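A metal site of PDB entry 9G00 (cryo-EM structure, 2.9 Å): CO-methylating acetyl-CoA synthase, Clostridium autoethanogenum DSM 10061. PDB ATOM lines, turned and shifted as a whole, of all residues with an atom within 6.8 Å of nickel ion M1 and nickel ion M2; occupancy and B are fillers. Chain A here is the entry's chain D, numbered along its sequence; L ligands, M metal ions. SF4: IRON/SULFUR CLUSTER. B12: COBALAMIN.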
ATOM      1  N   LEU A 487     -31.232 -31.983  15.345  1.00  0.00           N
ATOM      2  CA  LEU A 487     -29.912 -32.073  15.942  1.00  0.00           C
ATOM      3  C   LEU A 487     -29.751 -31.203  17.187  1.00  0.00           C
ATOM      4  O   LEU A 487     -28.738 -31.335  17.885  1.00  0.00           O
ATOM      5  CB  LEU A 487     -28.836 -31.694  14.928  1.00  0.00           C
ATOM      6  CG  LEU A 487     -27.835 -32.783  14.556  1.00  0.00           C
ATOM      7  CD1 LEU A 487     -26.806 -32.257  13.587  1.00  0.00           C
ATOM      8  CD2 LEU A 487     -27.144 -33.340  15.785  1.00  0.00           C
ATOM      9  N   CYS A 488     -30.692 -30.312  17.459  1.00  0.00           N
ATOM     10  CA  CYS A 488     -30.660 -29.493  18.664  1.00  0.00           C
ATOM     11  C   CYS A 488     -31.511 -30.059  19.781  1.00  0.00           C
ATOM     12  O   CYS A 488     -31.685 -29.397  20.813  1.00  0.00           O
ATOM     13  CB  CYS A 488     -31.109 -28.058  18.355  1.00  0.00           C
ATOM     14  SG  CYS A 488     -29.899 -27.072  17.438  1.00  0.00           S
ATOM     15  N   GLN A 489     -32.070 -31.260  19.602  1.00  0.00           N
ATOM     16  CA  GLN A 489     -32.847 -31.889  20.662  1.00  0.00           C
ATOM     17  C   GLN A 489     -31.982 -32.399  21.803  1.00  0.00           C
ATOM     18  O   GLN A 489     -32.533 -32.862  22.809  1.00  0.00           O
ATOM     19  CB  GLN A 489     -33.682 -33.033  20.097  1.00  0.00           C
ATOM     20  CG  GLN A 489     -34.793 -32.571  19.190  1.00  0.00           C
ATOM     21  CD  GLN A 489     -35.821 -33.651  18.935  1.00  0.00           C
ATOM     22  OE1 GLN A 489     -35.739 -34.735  19.501  1.00  0.00           O
ATOM     23  NE2 GLN A 489     -36.779 -33.363  18.072  1.00  0.00           N
ATOM     24  N   PHE A 491     -30.461 -30.626  23.818  1.00  0.00           N
ATOM     25  CA  PHE A 491     -30.777 -29.740  24.931  1.00  0.00           C
ATOM     26  C   PHE A 491     -32.161 -29.118  24.861  1.00  0.00           C
ATOM     27  O   PHE A 491     -32.597 -28.514  25.840  1.00  0.00           O
ATOM     28  CB  PHE A 491     -29.747 -28.606  25.025  1.00  0.00           C
ATOM     29  CG  PHE A 491     -29.779 -27.655  23.864  1.00  0.00           C
ATOM     30  CD1 PHE A 491     -29.140 -27.983  22.677  1.00  0.00           C
ATOM     31  CD2 PHE A 491     -30.421 -26.443  23.956  1.00  0.00           C
ATOM     32  CE1 PHE A 491     -29.162 -27.111  21.619  1.00  0.00           C
ATOM     33  CE2 PHE A 491     -30.431 -25.576  22.891  1.00  0.00           C
ATOM     34  CZ  PHE A 491     -29.803 -25.918  21.726  1.00  0.00           C
ATOM     35  N   ALA A 492     -32.866 -29.253  23.732  1.00  0.00           N
ATOM     36  CA  ALA A 492     -34.242 -28.779  23.587  1.00  0.00           C
ATOM     37  C   ALA A 492     -35.055 -29.955  23.059  1.00  0.00           C
ATOM     38  O   ALA A 492     -35.351 -30.038  21.864  1.00  0.00           O
ATOM     39  CB  ALA A 492     -34.323 -27.584  22.637  1.00  0.00           C
ATOM     40  N   HIS A 495     -37.936 -29.631  20.374  1.00  0.00           N
ATOM     41  CA  HIS A 495     -37.684 -28.754  19.246  1.00  0.00           C
ATOM     42  C   HIS A 495     -37.499 -29.547  17.954  1.00  0.00           C
ATOM     43  O   HIS A 495     -36.657 -30.453  17.888  1.00  0.00           O
ATOM     44  CB  HIS A 495     -36.435 -27.917  19.497  1.00  0.00           C
ATOM     45  CG  HIS A 495     -36.047 -27.064  18.326  1.00  0.00           C
ATOM     46  ND1 HIS A 495     -36.893 -26.128  17.781  1.00  0.00           N
ATOM     47  CD2 HIS A 495     -34.908 -27.027  17.594  1.00  0.00           C
ATOM     48  CE1 HIS A 495     -36.290 -25.538  16.767  1.00  0.00           C
ATOM     49  NE2 HIS A 495     -35.089 -26.061  16.633  1.00  0.00           N
ATOM     50  N   CYS A 497     -37.045 -28.485  13.809  1.00  0.00           N
ATOM     51  CA  CYS A 497     -36.867 -27.440  12.808  1.00  0.00           C
ATOM     52  C   CYS A 497     -37.438 -27.931  11.478  1.00  0.00           C
ATOM     53  O   CYS A 497     -36.992 -28.957  10.961  1.00  0.00           O
ATOM     54  CB  CYS A 497     -35.395 -27.077  12.632  1.00  0.00           C
ATOM     55  SG  CYS A 497     -34.763 -25.855  13.792  1.00  0.00           S
ATOM     56  N   LEU A 506     -32.865 -22.387  12.184  1.00  0.00           N
ATOM     57  CA  LEU A 506     -32.665 -21.287  13.118  1.00  0.00           C
ATOM     58  C   LEU A 506     -31.199 -20.950  13.267  1.00  0.00           C
ATOM     59  O   LEU A 506     -30.829 -19.767  13.337  1.00  0.00           O
ATOM     60  CB  LEU A 506     -33.275 -21.622  14.477  1.00  0.00           C
ATOM     61  CG  LEU A 506     -34.699 -22.164  14.476  1.00  0.00           C
ATOM     62  CD1 LEU A 506     -35.210 -22.224  15.896  1.00  0.00           C
ATOM     63  CD2 LEU A 506     -35.620 -21.316  13.615  1.00  0.00           C
ATOM     64  N   CYS A 507     -30.334 -21.959  13.314  1.00  0.00           N
ATOM     65  CA  CYS A 507     -28.905 -21.701  13.427  1.00  0.00           C
ATOM     66  C   CYS A 507     -28.348 -21.060  12.169  1.00  0.00           C
ATOM     67  O   CYS A 507     -27.278 -20.446  12.237  1.00  0.00           O
ATOM     68  CB  CYS A 507     -28.175 -23.008  13.705  1.00  0.00           C
ATOM     69  SG  CYS A 507     -28.571 -24.332  12.551  1.00  0.00           S
ATOM     70  N   SER A 573     -38.170 -22.896  19.296  1.00  0.00           N
ATOM     71  CA  SER A 573     -36.808 -22.419  19.163  1.00  0.00           C
ATOM     72  C   SER A 573     -35.910 -23.168  20.143  1.00  0.00           C
ATOM     73  O   SER A 573     -36.330 -23.481  21.256  1.00  0.00           O
ATOM     74  CB  SER A 573     -36.717 -20.925  19.446  1.00  0.00           C
ATOM     75  OG  SER A 573     -37.612 -20.192  18.626  1.00  0.00           O
ATOM     76  N   CYS A 574     -34.685 -23.447  19.707  1.00  0.00           N
ATOM     77  CA  CYS A 574     -33.742 -24.177  20.557  1.00  0.00           C
ATOM     78  C   CYS A 574     -32.875 -23.228  21.366  1.00  0.00           C
ATOM     79  O   CYS A 574     -32.998 -23.164  22.597  1.00  0.00           O
ATOM     80  CB  CYS A 574     -32.865 -25.094  19.697  1.00  0.00           C
ATOM     81  SG  CYS A 574     -32.493 -24.447  18.060  1.00  0.00           S
ATOM     82  N   GLY A 575     -32.082 -22.396  20.704  1.00  0.00           N
ATOM     83  CA  GLY A 575     -31.134 -21.563  21.424  1.00  0.00           C
ATOM     84  C   GLY A 575     -29.919 -21.184  20.618  1.00  0.00           C
ATOM     85  O   GLY A 575     -29.076 -20.402  21.067  1.00  0.00           O
ATOM     86  N   CYS A 576     -29.818 -21.750  19.422  1.00  0.00           N
ATOM     87  CA  CYS A 576     -28.772 -21.402  18.474  1.00  0.00           C
ATOM     88  C   CYS A 576     -29.097 -20.186  17.637  1.00  0.00           C
ATOM     89  O   CYS A 576     -28.209 -19.682  16.930  1.00  0.00           O
ATOM     90  CB  CYS A 576     -28.536 -22.597  17.560  1.00  0.00           C
ATOM     91  SG  CYS A 576     -30.056 -23.454  17.116  1.00  0.00           S
ATOM     92  N   PHE A 577     -30.323 -19.681  17.717  1.00  0.00           N
ATOM     93  CA  PHE A 577     -30.722 -18.538  16.903  1.00  0.00           C
ATOM     94  C   PHE A 577     -29.883 -17.310  17.217  1.00  0.00           C
ATOM     95  O   PHE A 577     -29.554 -17.046  18.374  1.00  0.00           O
ATOM     96  CB  PHE A 577     -32.207 -18.240  17.122  1.00  0.00           C
ATOM     97  CG  PHE A 577     -32.624 -18.277  18.563  1.00  0.00           C
ATOM     98  CD1 PHE A 577     -32.397 -17.202  19.400  1.00  0.00           C
ATOM     99  CD2 PHE A 577     -33.235 -19.395  19.086  1.00  0.00           C
ATOM    100  CE1 PHE A 577     -32.775 -17.251  20.724  1.00  0.00           C
ATOM    101  CE2 PHE A 577     -33.616 -19.441  20.401  1.00  0.00           C
ATOM    102  CZ  PHE A 577     -33.389 -18.372  21.225  1.00  0.00           C
ATOM    103  N   ARG A 595     -28.054 -11.493  18.609  1.00  0.00           N
ATOM    104  CA  ARG A 595     -27.386 -12.017  19.800  1.00  0.00           C
ATOM    105  C   ARG A 595     -26.286 -11.076  20.283  1.00  0.00           C
ATOM    106  O   ARG A 595     -26.152 -10.850  21.493  1.00  0.00           O
ATOM    107  CB  ARG A 595     -26.827 -13.400  19.512  1.00  0.00           C
ATOM    108  CG  ARG A 595     -26.075 -14.020  20.675  1.00  0.00           C
ATOM    109  CD  ARG A 595     -25.696 -15.470  20.391  1.00  0.00           C
ATOM    110  NE  ARG A 595     -26.860 -16.337  20.345  1.00  0.00           N
ATOM    111  CZ  ARG A 595     -27.400 -16.925  21.404  1.00  0.00           C
ATOM    112  NH1 ARG A 595     -26.909 -16.747  22.620  1.00  0.00           N
ATOM    113  NH2 ARG A 595     -28.465 -17.714  21.240  1.00  0.00           N
ATOM    114  N   GLY A 615     -36.379 -19.766  23.786  1.00  0.00           N
ATOM    115  CA  GLY A 615     -35.654 -20.995  23.571  1.00  0.00           C
ATOM    116  C   GLY A 615     -36.171 -22.144  24.407  1.00  0.00           C
ATOM    117  O   GLY A 615     -37.103 -22.019  25.202  1.00  0.00           O
HETATM  118 FE1  SF4 L   1     -30.725 -28.728  13.160  1.00  0.00          FE
HETATM  119 FE2  SF4 L   1     -32.609 -26.791  13.592  1.00  0.00          FE
HETATM  120 FE3  SF4 L   1     -30.065 -26.088  12.878  1.00  0.00          FE
HETATM  121 FE4  SF4 L   1     -30.558 -27.130  15.365  1.00  0.00          FE
HETATM  122  S1  SF4 L   1     -31.337 -25.153  14.534  1.00  0.00           S
HETATM  123  S2  SF4 L   1     -28.860 -27.701  13.956  1.00  0.00           S
HETATM  124  S3  SF4 L   1     -32.208 -28.625  14.890  1.00  0.00           S
HETATM  125  S4  SF4 L   1     -31.558 -27.265  11.625  1.00  0.00           S
HETATM  126 CO   B12 L   2     -24.409 -25.036  18.157  1.00  0.00          CO
HETATM  127  N21 B12 L   2     -23.733 -25.610  16.507  1.00  0.00           N
HETATM  128  N22 B12 L   2     -24.333 -23.201  17.574  1.00  0.00           N
HETATM  129  N23 B12 L   2     -25.099 -24.758  19.855  1.00  0.00           N
HETATM  130  N24 B12 L   2     -24.400 -26.919  18.484  1.00  0.00           N
HETATM  131  C1  B12 L   2     -23.394 -27.040  16.298  1.00  0.00           C
HETATM  132  C20 B12 L   2     -21.921 -27.297  16.775  1.00  0.00           C
HETATM  133  C2  B12 L   2     -23.528 -27.209  14.742  1.00  0.00           C
HETATM  134  C25 B12 L   2     -22.824 -28.487  14.172  1.00  0.00           C
HETATM  135  C26 B12 L   2     -25.019 -27.173  14.351  1.00  0.00           C
HETATM  136  C27 B12 L   2     -25.221 -27.247  12.839  1.00  0.00           C
HETATM  137  O28 B12 L   2     -24.695 -28.060  12.079  1.00  0.00           O
HETATM  138  N29 B12 L   2     -26.061 -26.320  12.366  1.00  0.00           N
HETATM  139  C3  B12 L   2     -22.881 -25.868  14.294  1.00  0.00           C
HETATM  140  C30 B12 L   2     -21.352 -25.719  14.024  1.00  0.00           C
HETATM  141  C31 B12 L   2     -21.014 -25.181  12.594  1.00  0.00           C
HETATM  142  C32 B12 L   2     -19.633 -24.553  12.451  1.00  0.00           C
HETATM  143  O34 B12 L   2     -19.153 -23.862  13.359  1.00  0.00           O
HETATM  144  N33 B12 L   2     -18.952 -24.775  11.320  1.00  0.00           N
HETATM  145  C4  B12 L   2     -23.321 -24.938  15.442  1.00  0.00           C
HETATM  146  C5  B12 L   2     -23.417 -23.495  15.316  1.00  0.00           C
HETATM  147  C35 B12 L   2     -22.943 -22.969  13.991  1.00  0.00           C
HETATM  148  C6  B12 L   2     -23.886 -22.678  16.335  1.00  0.00           C
HETATM  149  C7  B12 L   2     -24.028 -21.157  16.330  1.00  0.00           C
HETATM  150  C36 B12 L   2     -22.706 -20.421  16.010  1.00  0.00           C
HETATM  151  C37 B12 L   2     -25.160 -20.750  15.300  1.00  0.00           C
HETATM  152  C38 B12 L   2     -25.296 -19.193  15.172  1.00  0.00           C
HETATM  153  O39 B12 L   2     -24.816 -18.663  14.191  1.00  0.00           O
HETATM  154  N40 B12 L   2     -25.930 -18.471  16.092  1.00  0.00           N
HETATM  155  C8  B12 L   2     -24.559 -20.834  17.733  1.00  0.00           C
HETATM  156  C41 B12 L   2     -23.594 -19.945  18.622  1.00  0.00           C
HETATM  157  C42 B12 L   2     -24.258 -19.341  19.868  1.00  0.00           C
HETATM  158  C43 B12 L   2     -23.478 -18.202  20.427  1.00  0.00           C
HETATM  159  O44 B12 L   2     -22.761 -17.509  19.677  1.00  0.00           O
HETATM  160  N45 B12 L   2     -23.511 -17.910  21.739  1.00  0.00           N
HETATM  161  C9  B12 L   2     -24.723 -22.216  18.347  1.00  0.00           C
HETATM  162  C10 B12 L   2     -25.190 -22.387  19.614  1.00  0.00           C
HETATM  163  C11 B12 L   2     -25.372 -23.517  20.320  1.00  0.00           C
HETATM  164  C12 B12 L   2     -25.992 -23.521  21.708  1.00  0.00           C
HETATM  165  C46 B12 L   2     -27.473 -23.053  21.518  1.00  0.00           C
HETATM  166  C47 B12 L   2     -25.233 -22.547  22.651  1.00  0.00           C
HETATM  167  C13 B12 L   2     -25.887 -24.977  22.093  1.00  0.00           C
HETATM  168  C48 B12 L   2     -24.847 -25.308  23.235  1.00  0.00           C
HETATM  169  C49 B12 L   2     -25.560 -25.490  24.583  1.00  0.00           C
HETATM  170  C50 B12 L   2     -24.690 -26.436  25.416  1.00  0.00           C
HETATM  171  O51 B12 L   2     -23.417 -26.271  25.483  1.00  0.00           O
HETATM  172  N52 B12 L   2     -25.321 -27.389  25.992  1.00  0.00           N
HETATM  173  C14 B12 L   2     -25.411 -25.664  20.827  1.00  0.00           C
HETATM  174  C15 B12 L   2     -25.259 -27.033  20.715  1.00  0.00           C
HETATM  175  C53 B12 L   2     -25.631 -27.954  21.869  1.00  0.00           C
HETATM  176  C16 B12 L   2     -24.691 -27.615  19.543  1.00  0.00           C
HETATM  177  C17 B12 L   2     -24.604 -29.127  19.215  1.00  0.00           C
HETATM  178  C54 B12 L   2     -26.106 -29.512  19.117  1.00  0.00           C
HETATM  179  C55 B12 L   2     -23.936 -30.055  20.201  1.00  0.00           C
HETATM  180  C56 B12 L   2     -22.557 -29.657  20.746  1.00  0.00           C
HETATM  181  C57 B12 L   2     -21.970 -30.822  21.555  1.00  0.00           C
HETATM  182  O58 B12 L   2     -22.220 -30.937  22.746  1.00  0.00           O
HETATM  183  N59 B12 L   2     -21.252 -31.701  20.886  1.00  0.00           N
HETATM  184  C18 B12 L   2     -23.930 -29.136  17.848  1.00  0.00           C
HETATM  185  C60 B12 L   2     -24.249 -30.327  16.891  1.00  0.00           C
HETATM  186  C61 B12 L   2     -23.008 -31.080  16.409  1.00  0.00           C
HETATM  187  O63 B12 L   2     -21.929 -31.028  17.014  1.00  0.00           O
HETATM  188  N62 B12 L   2     -23.207 -31.784  15.301  1.00  0.00           N
HETATM  189  C19 B12 L   2     -24.332 -27.791  17.271  1.00  0.00           C
HETATM  190  C1P B12 L   2     -20.671 -32.902  21.519  1.00  0.00           C
HETATM  191  C2P B12 L   2     -19.486 -32.586  22.435  1.00  0.00           C
HETATM  192  C3P B12 L   2     -19.243 -33.723  23.438  1.00  0.00           C
HETATM  193  O3  B12 L   2     -18.318 -32.547  21.572  1.00  0.00           O
HETATM  194  O4  B12 L   2     -17.542 -30.557  22.916  1.00  0.00           O
HETATM  195  O5  B12 L   2     -16.417 -31.193  20.657  1.00  0.00           O
HETATM  196  P   B12 L   2     -17.076 -31.583  21.970  1.00  0.00           P
HETATM  197  O2  B12 L   2     -16.018 -32.579  22.733  1.00  0.00           O
HETATM  198  C3R B12 L   2     -15.466 -33.708  22.123  1.00  0.00           C
HETATM  199  C2R B12 L   2     -14.165 -33.450  21.368  1.00  0.00           C
HETATM  200  O7R B12 L   2     -13.771 -32.115  21.282  1.00  0.00           O
HETATM  201  C1R B12 L   2     -13.091 -34.327  22.089  1.00  0.00           C
HETATM  202  O6R B12 L   2     -13.807 -35.220  22.892  1.00  0.00           O
HETATM  203  C4R B12 L   2     -15.036 -34.613  23.320  1.00  0.00           C
HETATM  204  C5R B12 L   2     -16.049 -35.692  23.694  1.00  0.00           C
HETATM  205  O8R B12 L   2     -16.118 -36.656  22.596  1.00  0.00           O
HETATM  206  N1B B12 L   2     -12.117 -33.623  22.932  1.00  0.00           N
HETATM  207  C8B B12 L   2     -10.817 -34.054  23.075  1.00  0.00           C
HETATM  208  C2B B12 L   2     -12.228 -32.545  23.697  1.00  0.00           C
HETATM  209  N3B B12 L   2     -11.098 -32.234  24.308  1.00  0.00           N
HETATM  210  C9B B12 L   2     -10.153 -33.201  23.931  1.00  0.00           C
HETATM  211  C4B B12 L   2      -8.801 -33.439  24.222  1.00  0.00           C
HETATM  212  C5B B12 L   2      -8.138 -34.525  23.655  1.00  0.00           C
HETATM  213  C5M B12 L   2      -6.686 -34.804  23.964  1.00  0.00           C
HETATM  214  C6B B12 L   2      -8.805 -35.404  22.779  1.00  0.00           C
HETATM  215  C6M B12 L   2      -8.192 -36.586  22.130  1.00  0.00           C
HETATM  216  C7B B12 L   2     -10.163 -35.149  22.496  1.00  0.00           C
HETATM  217 NI    NI M   1     -31.180 -22.958  18.981  1.00  0.00          NI
HETATM  218 NI    NI M   2     -30.935 -25.284  16.863  1.00  0.00          NI
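Phe 577 touches nickel ion M1 (N to NI, 3.6 Å).
Four residues have an atom within 4 Å of nickel ion M1: Cys 574, Gly 575, Cys 576 and Phe 577.
The backbone carbonyl oxygen (O) of Phe 577 lies within hydrogen-bond range of the guanidinium group (NH2) of Arg 595 (3.1 Å).
A ring nitrogen (NE2) of His 495 lies close to the side-chain sulfur (SG) of Cys 574.
NH2 of Arg 595 lies within hydrogen-bond range of O of Gly 575.
Nickel ion M2 is bound by the side-chain sulfur (SG) of Cys 576 (2.0 Å), the side-chain sulfur (SG) of Cys 574 (2.1 Å), the side-chain sulfur (SG) of Cys 488 (2.1 Å) and a sulfur (S1) of SF4 L1 (2.4 Å).
Of the 16 residues printed, 3 come within 4 Å of nickel ion M2.
The nearest printed residue that does not touch nickel ion M2 is His 495 (4.2 Å).
S2 of SF4 L1 sits close to N29 of B12 L2 (3.5 Å).
Nickel ion M1 is bound by N of Cys 576 (1.9 Å).
N of Gly 575 is bound to nickel ion M1 (2.0 Å).
SG of Cys 574 binds nickel ion M1, at 2.2 Å.
SG of Cys 576 binds nickel ion M1, at 2.2 Å.
Nickel ion M1 has four donor atoms within binding distance.
O of Cys 576 sits at hydrogen-bond distance from N40 of B12 L2 (2.7 Å).
An iron atom (FE2) of SF4 L1 is bound by the side-chain sulfur of Cys 497, 2.4 Å away.
The side-chain sulfur (SG) of Cys 507 sits close to a nitrogen (N29) of B12 L2 (3.2 Å).
The side-chain sulfur (SG) of Cys 507 binds an iron atom (FE3) of SF4 L1.
The backbone NH (N) of Cys 507 sits close to a sulfur (S1) of SF4 L1 (3.6 Å).
FE4 of SF4 L1 is bound by SG of Cys 488 (2.2 Å).
The backbone NH (N) of Leu 487 lies close to a sulfur (S3) of SF4 L1.
The backbone NH (N) of Cys 488 lies close to a sulfur (S3) of SF4 L1 (3.4 Å).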
